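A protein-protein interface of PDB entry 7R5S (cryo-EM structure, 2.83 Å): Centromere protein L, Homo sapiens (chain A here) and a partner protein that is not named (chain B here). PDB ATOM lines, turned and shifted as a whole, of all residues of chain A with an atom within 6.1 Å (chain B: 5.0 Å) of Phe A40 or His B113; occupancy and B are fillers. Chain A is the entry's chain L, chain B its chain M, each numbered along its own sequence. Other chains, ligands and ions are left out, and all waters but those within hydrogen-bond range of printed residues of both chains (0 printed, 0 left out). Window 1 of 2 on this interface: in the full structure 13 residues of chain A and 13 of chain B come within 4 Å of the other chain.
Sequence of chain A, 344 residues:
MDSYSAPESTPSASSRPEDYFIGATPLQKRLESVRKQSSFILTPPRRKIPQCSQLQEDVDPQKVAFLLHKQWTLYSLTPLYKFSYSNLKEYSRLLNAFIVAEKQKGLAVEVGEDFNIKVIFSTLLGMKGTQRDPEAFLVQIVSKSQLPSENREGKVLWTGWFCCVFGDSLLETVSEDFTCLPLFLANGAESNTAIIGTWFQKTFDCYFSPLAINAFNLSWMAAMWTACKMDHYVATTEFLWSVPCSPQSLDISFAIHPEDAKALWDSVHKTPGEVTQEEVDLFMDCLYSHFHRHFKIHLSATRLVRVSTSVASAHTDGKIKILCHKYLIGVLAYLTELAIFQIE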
ATOM      1  N   SER A  38      -0.523  -4.257  -2.728  1.00  0.00           N
ATOM      2  CA  SER A  38       0.055  -4.105  -4.063  1.00  0.00           C
ATOM      3  C   SER A  38       0.917  -5.327  -4.371  1.00  0.00           C
ATOM      4  O   SER A  38       2.138  -5.337  -4.195  1.00  0.00           O
ATOM      5  CB  SER A  38       0.857  -2.814  -4.157  1.00  0.00           C
ATOM      6  OG  SER A  38       1.797  -2.876  -5.216  1.00  0.00           O
ATOM      7  N   SER A  39       0.257  -6.379  -4.842  1.00  0.00           N
ATOM      8  CA  SER A  39       0.912  -7.611  -5.253  1.00  0.00           C
ATOM      9  C   SER A  39       0.848  -7.754  -6.769  1.00  0.00           C
ATOM     10  O   SER A  39       0.157  -7.004  -7.462  1.00  0.00           O
ATOM     11  CB  SER A  39       0.270  -8.824  -4.570  1.00  0.00           C
ATOM     12  OG  SER A  39       1.094  -9.970  -4.686  1.00  0.00           O
ATOM     13  N   PHE A  40       1.585  -8.741  -7.282  1.00  0.00           N
ATOM     14  CA  PHE A  40       1.646  -9.013  -8.712  1.00  0.00           C
ATOM     15  C   PHE A  40       0.807 -10.224  -9.109  1.00  0.00           C
ATOM     16  O   PHE A  40       1.170 -10.954 -10.037  1.00  0.00           O
ATOM     17  CB  PHE A  40       3.097  -9.202  -9.155  1.00  0.00           C
ATOM     18  CG  PHE A  40       3.924  -7.952  -9.068  1.00  0.00           C
ATOM     19  CD1 PHE A  40       3.809  -6.963 -10.031  1.00  0.00           C
ATOM     20  CD2 PHE A  40       4.815  -7.765  -8.025  1.00  0.00           C
ATOM     21  CE1 PHE A  40       4.567  -5.811  -9.954  1.00  0.00           C
ATOM     22  CE2 PHE A  40       5.577  -6.615  -7.944  1.00  0.00           C
ATOM     23  CZ  PHE A  40       5.452  -5.637  -8.910  1.00  0.00           C
ATOM     24  N   ILE A  41      -0.308 -10.449  -8.424  1.00  0.00           N
ATOM     25  CA  ILE A  41      -1.201 -11.559  -8.727  1.00  0.00           C
ATOM     26  C   ILE A  41      -2.422 -11.098  -9.513  1.00  0.00           C
ATOM     27  O   ILE A  41      -2.851 -11.774 -10.449  1.00  0.00           O
ATOM     28  CB  ILE A  41      -1.615 -12.278  -7.425  1.00  0.00           C
ATOM     29  CG1 ILE A  41      -0.381 -12.812  -6.695  1.00  0.00           C
ATOM     30  CG2 ILE A  41      -2.587 -13.411  -7.722  1.00  0.00           C
ATOM     31  CD1 ILE A  41       0.392 -13.847  -7.480  1.00  0.00           C
ATOM     32  N   LEU A  42      -2.986  -9.950  -9.151  1.00  0.00           N
ATOM     33  CA  LEU A  42      -4.173  -9.443  -9.818  1.00  0.00           C
ATOM     34  C   LEU A  42      -3.833  -8.929 -11.212  1.00  0.00           C
ATOM     35  O   LEU A  42      -2.749  -8.393 -11.455  1.00  0.00           O
ATOM     36  CB  LEU A  42      -4.820  -8.326  -8.997  1.00  0.00           C
ATOM     37  CG  LEU A  42      -5.421  -8.692  -7.636  1.00  0.00           C
ATOM     38  CD1 LEU A  42      -6.096 -10.056  -7.686  1.00  0.00           C
ATOM     39  CD2 LEU A  42      -4.375  -8.639  -6.527  1.00  0.00           C
ATOM     40  N   PRO A  44      -3.821  -6.421 -14.238  1.00  0.00           N
ATOM     41  CA  PRO A  44      -3.983  -4.976 -14.372  1.00  0.00           C
ATOM     42  C   PRO A  44      -5.215  -4.646 -15.195  1.00  0.00           C
ATOM     43  O   PRO A  44      -5.552  -5.367 -16.151  1.00  0.00           O
ATOM     44  CB  PRO A  44      -2.694  -4.538 -15.089  1.00  0.00           C
ATOM     45  CG  PRO A  44      -1.719  -5.638 -14.831  1.00  0.00           C
ATOM     46  CD  PRO A  44      -2.539  -6.888 -14.791  1.00  0.00           C
ATOM     47  N   PHE A 216       7.222   0.622 -20.953  1.00  0.00           N
ATOM     48  CA  PHE A 216       5.849   0.140 -20.837  1.00  0.00           C
ATOM     49  C   PHE A 216       4.862   1.303 -20.812  1.00  0.00           C
ATOM     50  O   PHE A 216       3.901   1.345 -21.594  1.00  0.00           O
ATOM     51  CB  PHE A 216       5.719  -0.719 -19.577  1.00  0.00           C
ATOM     52  CG  PHE A 216       4.390  -1.402 -19.430  1.00  0.00           C
ATOM     53  CD1 PHE A 216       4.117  -2.571 -20.117  1.00  0.00           C
ATOM     54  CD2 PHE A 216       3.423  -0.886 -18.584  1.00  0.00           C
ATOM     55  CE1 PHE A 216       2.898  -3.204 -19.976  1.00  0.00           C
ATOM     56  CE2 PHE A 216       2.203  -1.515 -18.439  1.00  0.00           C
ATOM     57  CZ  PHE A 216       1.940  -2.675 -19.136  1.00  0.00           C
ATOM     58  N   PHE A 341       1.936   6.104  -7.242  1.00  0.00           N
ATOM     59  CA  PHE A 341       2.476   4.750  -7.187  1.00  0.00           C
ATOM     60  C   PHE A 341       3.934   4.755  -6.746  1.00  0.00           C
ATOM     61  O   PHE A 341       4.380   3.832  -6.055  1.00  0.00           O
ATOM     62  CB  PHE A 341       2.331   4.062  -8.543  1.00  0.00           C
ATOM     63  CG  PHE A 341       2.924   2.681  -8.586  1.00  0.00           C
ATOM     64  CD1 PHE A 341       2.224   1.599  -8.080  1.00  0.00           C
ATOM     65  CD2 PHE A 341       4.180   2.467  -9.128  1.00  0.00           C
ATOM     66  CE1 PHE A 341       2.767   0.328  -8.114  1.00  0.00           C
ATOM     67  CE2 PHE A 341       4.727   1.198  -9.164  1.00  0.00           C
ATOM     68  CZ  PHE A 341       4.019   0.128  -8.657  1.00  0.00           C
ATOM     69  N   SER B 111      10.734  -3.207 -20.229  1.00  0.00           N
ATOM     70  CA  SER B 111       9.646  -3.101 -21.190  1.00  0.00           C
ATOM     71  C   SER B 111       8.551  -4.131 -20.953  1.00  0.00           C
ATOM     72  O   SER B 111       7.523  -4.092 -21.635  1.00  0.00           O
ATOM     73  CB  SER B 111      10.187  -3.243 -22.616  1.00  0.00           C
ATOM     74  OG  SER B 111       9.135  -3.442 -23.541  1.00  0.00           O
ATOM     75  N   ILE B 112       8.747  -5.046 -20.007  1.00  0.00           N
ATOM     76  CA  ILE B 112       7.792  -6.105 -19.705  1.00  0.00           C
ATOM     77  C   ILE B 112       7.417  -6.004 -18.233  1.00  0.00           C
ATOM     78  O   ILE B 112       8.295  -5.880 -17.372  1.00  0.00           O
ATOM     79  CB  ILE B 112       8.369  -7.496 -20.027  1.00  0.00           C
ATOM     80  CG1 ILE B 112       8.816  -7.564 -21.487  1.00  0.00           C
ATOM     81  CG2 ILE B 112       7.347  -8.581 -19.730  1.00  0.00           C
ATOM     82  CD1 ILE B 112       9.473  -8.871 -21.862  1.00  0.00           C
ATOM     83  N   HIS B 113       6.120  -6.054 -17.951  1.00  0.00           N
ATOM     84  CA  HIS B 113       5.649  -6.016 -16.574  1.00  0.00           C
ATOM     85  C   HIS B 113       5.983  -7.321 -15.860  1.00  0.00           C
ATOM     86  O   HIS B 113       6.043  -8.393 -16.468  1.00  0.00           O
ATOM     87  CB  HIS B 113       4.143  -5.766 -16.534  1.00  0.00           C
ATOM     88  CG  HIS B 113       3.687  -5.005 -15.327  1.00  0.00           C
ATOM     89  ND1 HIS B 113       3.259  -5.627 -14.174  1.00  0.00           N
ATOM     90  CD2 HIS B 113       3.588  -3.675 -15.096  1.00  0.00           C
ATOM     91  CE1 HIS B 113       2.919  -4.711 -13.283  1.00  0.00           C
ATOM     92  NE2 HIS B 113       3.109  -3.520 -13.818  1.00  0.00           N
ATOM     93  N   ARG B 114       6.209  -7.221 -14.547  1.00  0.00           N
ATOM     94  CA  ARG B 114       6.537  -8.408 -13.763  1.00  0.00           C
ATOM     95  C   ARG B 114       5.339  -9.340 -13.622  1.00  0.00           C
ATOM     96  O   ARG B 114       5.516 -10.551 -13.433  1.00  0.00           O
ATOM     97  CB  ARG B 114       7.061  -8.002 -12.387  1.00  0.00           C
ATOM     98  CG  ARG B 114       8.426  -7.335 -12.420  1.00  0.00           C
ATOM     99  CD  ARG B 114       8.815  -6.791 -11.056  1.00  0.00           C
ATOM    100  NE  ARG B 114       8.709  -7.804 -10.011  1.00  0.00           N
ATOM    101  CZ  ARG B 114       9.026  -7.597  -8.738  1.00  0.00           C
ATOM    102  NH1 ARG B 114       9.470  -6.410  -8.348  1.00  0.00           N
ATOM    103  NH2 ARG B 114       8.898  -8.576  -7.853  1.00  0.00           N
ATOM    104  N   HIS B 115       4.121  -8.801 -13.711  1.00  0.00           N
ATOM    105  CA  HIS B 115       2.935  -9.649 -13.654  1.00  0.00           C
ATOM    106  C   HIS B 115       2.915 -10.654 -14.797  1.00  0.00           C
ATOM    107  O   HIS B 115       2.438 -11.780 -14.622  1.00  0.00           O
ATOM    108  CB  HIS B 115       1.672  -8.788 -13.681  1.00  0.00           C
ATOM    109  CG  HIS B 115       0.419  -9.564 -13.948  1.00  0.00           C
ATOM    110  ND1 HIS B 115      -0.155 -10.396 -13.011  1.00  0.00           N
ATOM    111  CD2 HIS B 115      -0.366  -9.639 -15.049  1.00  0.00           C
ATOM    112  CE1 HIS B 115      -1.241 -10.947 -13.520  1.00  0.00           C
ATOM    113  NE2 HIS B 115      -1.392 -10.504 -14.756  1.00  0.00           N
ATOM    114  N   THR B 116       3.447 -10.276 -15.961  1.00  0.00           N
ATOM    115  CA  THR B 116       3.468 -11.186 -17.102  1.00  0.00           C
ATOM    116  C   THR B 116       4.303 -12.425 -16.804  1.00  0.00           C
ATOM    117  O   THR B 116       3.840 -13.558 -16.986  1.00  0.00           O
ATOM    118  CB  THR B 116       4.002 -10.462 -18.339  1.00  0.00           C
ATOM    119  OG1 THR B 116       3.155  -9.347 -18.644  1.00  0.00           O
ATOM    120  CG2 THR B 116       4.039 -11.403 -19.532  1.00  0.00           C
ATOM    121  N   VAL B 117       5.538 -12.233 -16.335  1.00  0.00           N
ATOM    122  CA  VAL B 117       6.393 -13.382 -16.052  1.00  0.00           C
ATOM    123  C   VAL B 117       5.895 -14.140 -14.828  1.00  0.00           C
ATOM    124  O   VAL B 117       6.048 -15.365 -14.749  1.00  0.00           O
ATOM    125  CB  VAL B 117       7.862 -12.947 -15.894  1.00  0.00           C
ATOM    126  CG1 VAL B 117       8.411 -12.450 -17.222  1.00  0.00           C
ATOM    127  CG2 VAL B 117       8.000 -11.878 -14.827  1.00  0.00           C
ATOM    128  N   VAL B 118       5.273 -13.448 -13.869  1.00  0.00           N
ATOM    129  CA  VAL B 118       4.698 -14.140 -12.717  1.00  0.00           C
ATOM    130  C   VAL B 118       3.591 -15.088 -13.167  1.00  0.00           C
ATOM    131  O   VAL B 118       3.544 -16.257 -12.764  1.00  0.00           O
ATOM    132  CB  VAL B 118       4.190 -13.125 -11.678  1.00  0.00           C
ATOM    133  CG1 VAL B 118       3.212 -13.787 -10.721  1.00  0.00           C
ATOM    134  CG2 VAL B 118       5.356 -12.529 -10.909  1.00  0.00           C
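The backbone carbonyl oxygen of Phe A40 sits at hydrogen-bond distance from a ring nitrogen (ND1) of His B115, 3.3 Å away.
A ring nitrogen (ND1) of His B113 lies close to the backbone NH (N) of His B115 (3.3 Å).
Phe A40 touches His B113.
Arg B114 touches Phe A40 (CZ to CE2, 3.7 Å).
Phe A40 touches Val B118.
His B115 touches Ile A41 (CE1 to O, 3.6 Å).
His B115 touches Leu A42.
Pro A44 touches His B115 (CD to CD2, 3.5 Å).
Of the printed residues of chain A, Val B118 touches Phe A40.
Printed residues of chain A within 4 Å of Arg B114: Phe A40.
Of the printed residues of chain B, Pro A44 touches His B115 (3.5 Å).
Printed residues of chain A within 4 Å of His B115: Phe A40, Ile A41, Leu A42 and Pro A44.
Of the printed residues of chain B, Leu A42 touches His B115 (3.6 Å).
The nearest residue of chain A that does not touch His B113 is Phe A216 (4.2 Å).
Of the 8 printed residues of chain A, 4 touch a printed residue of chain B.
Printed residues of chain A that touch a printed residue of chain B: Phe A40, Ile A41, Leu A42 and Pro A44.
Of the 8 printed residues of chain B, 4 touch a printed residue of chain A.
Printed residues of chain B that touch a printed residue of chain A: His B113, Arg B114, His B115 and Val B118.
Hydrophobic or aromatic side chains of chain B that line the printed part of chain A: His B113, His B115 and Val B118.
Along chain B the printed residues that touch a printed residue of chain A span positions 113 to 118.
Among the printed residues, 7 pairs touch across the chains.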
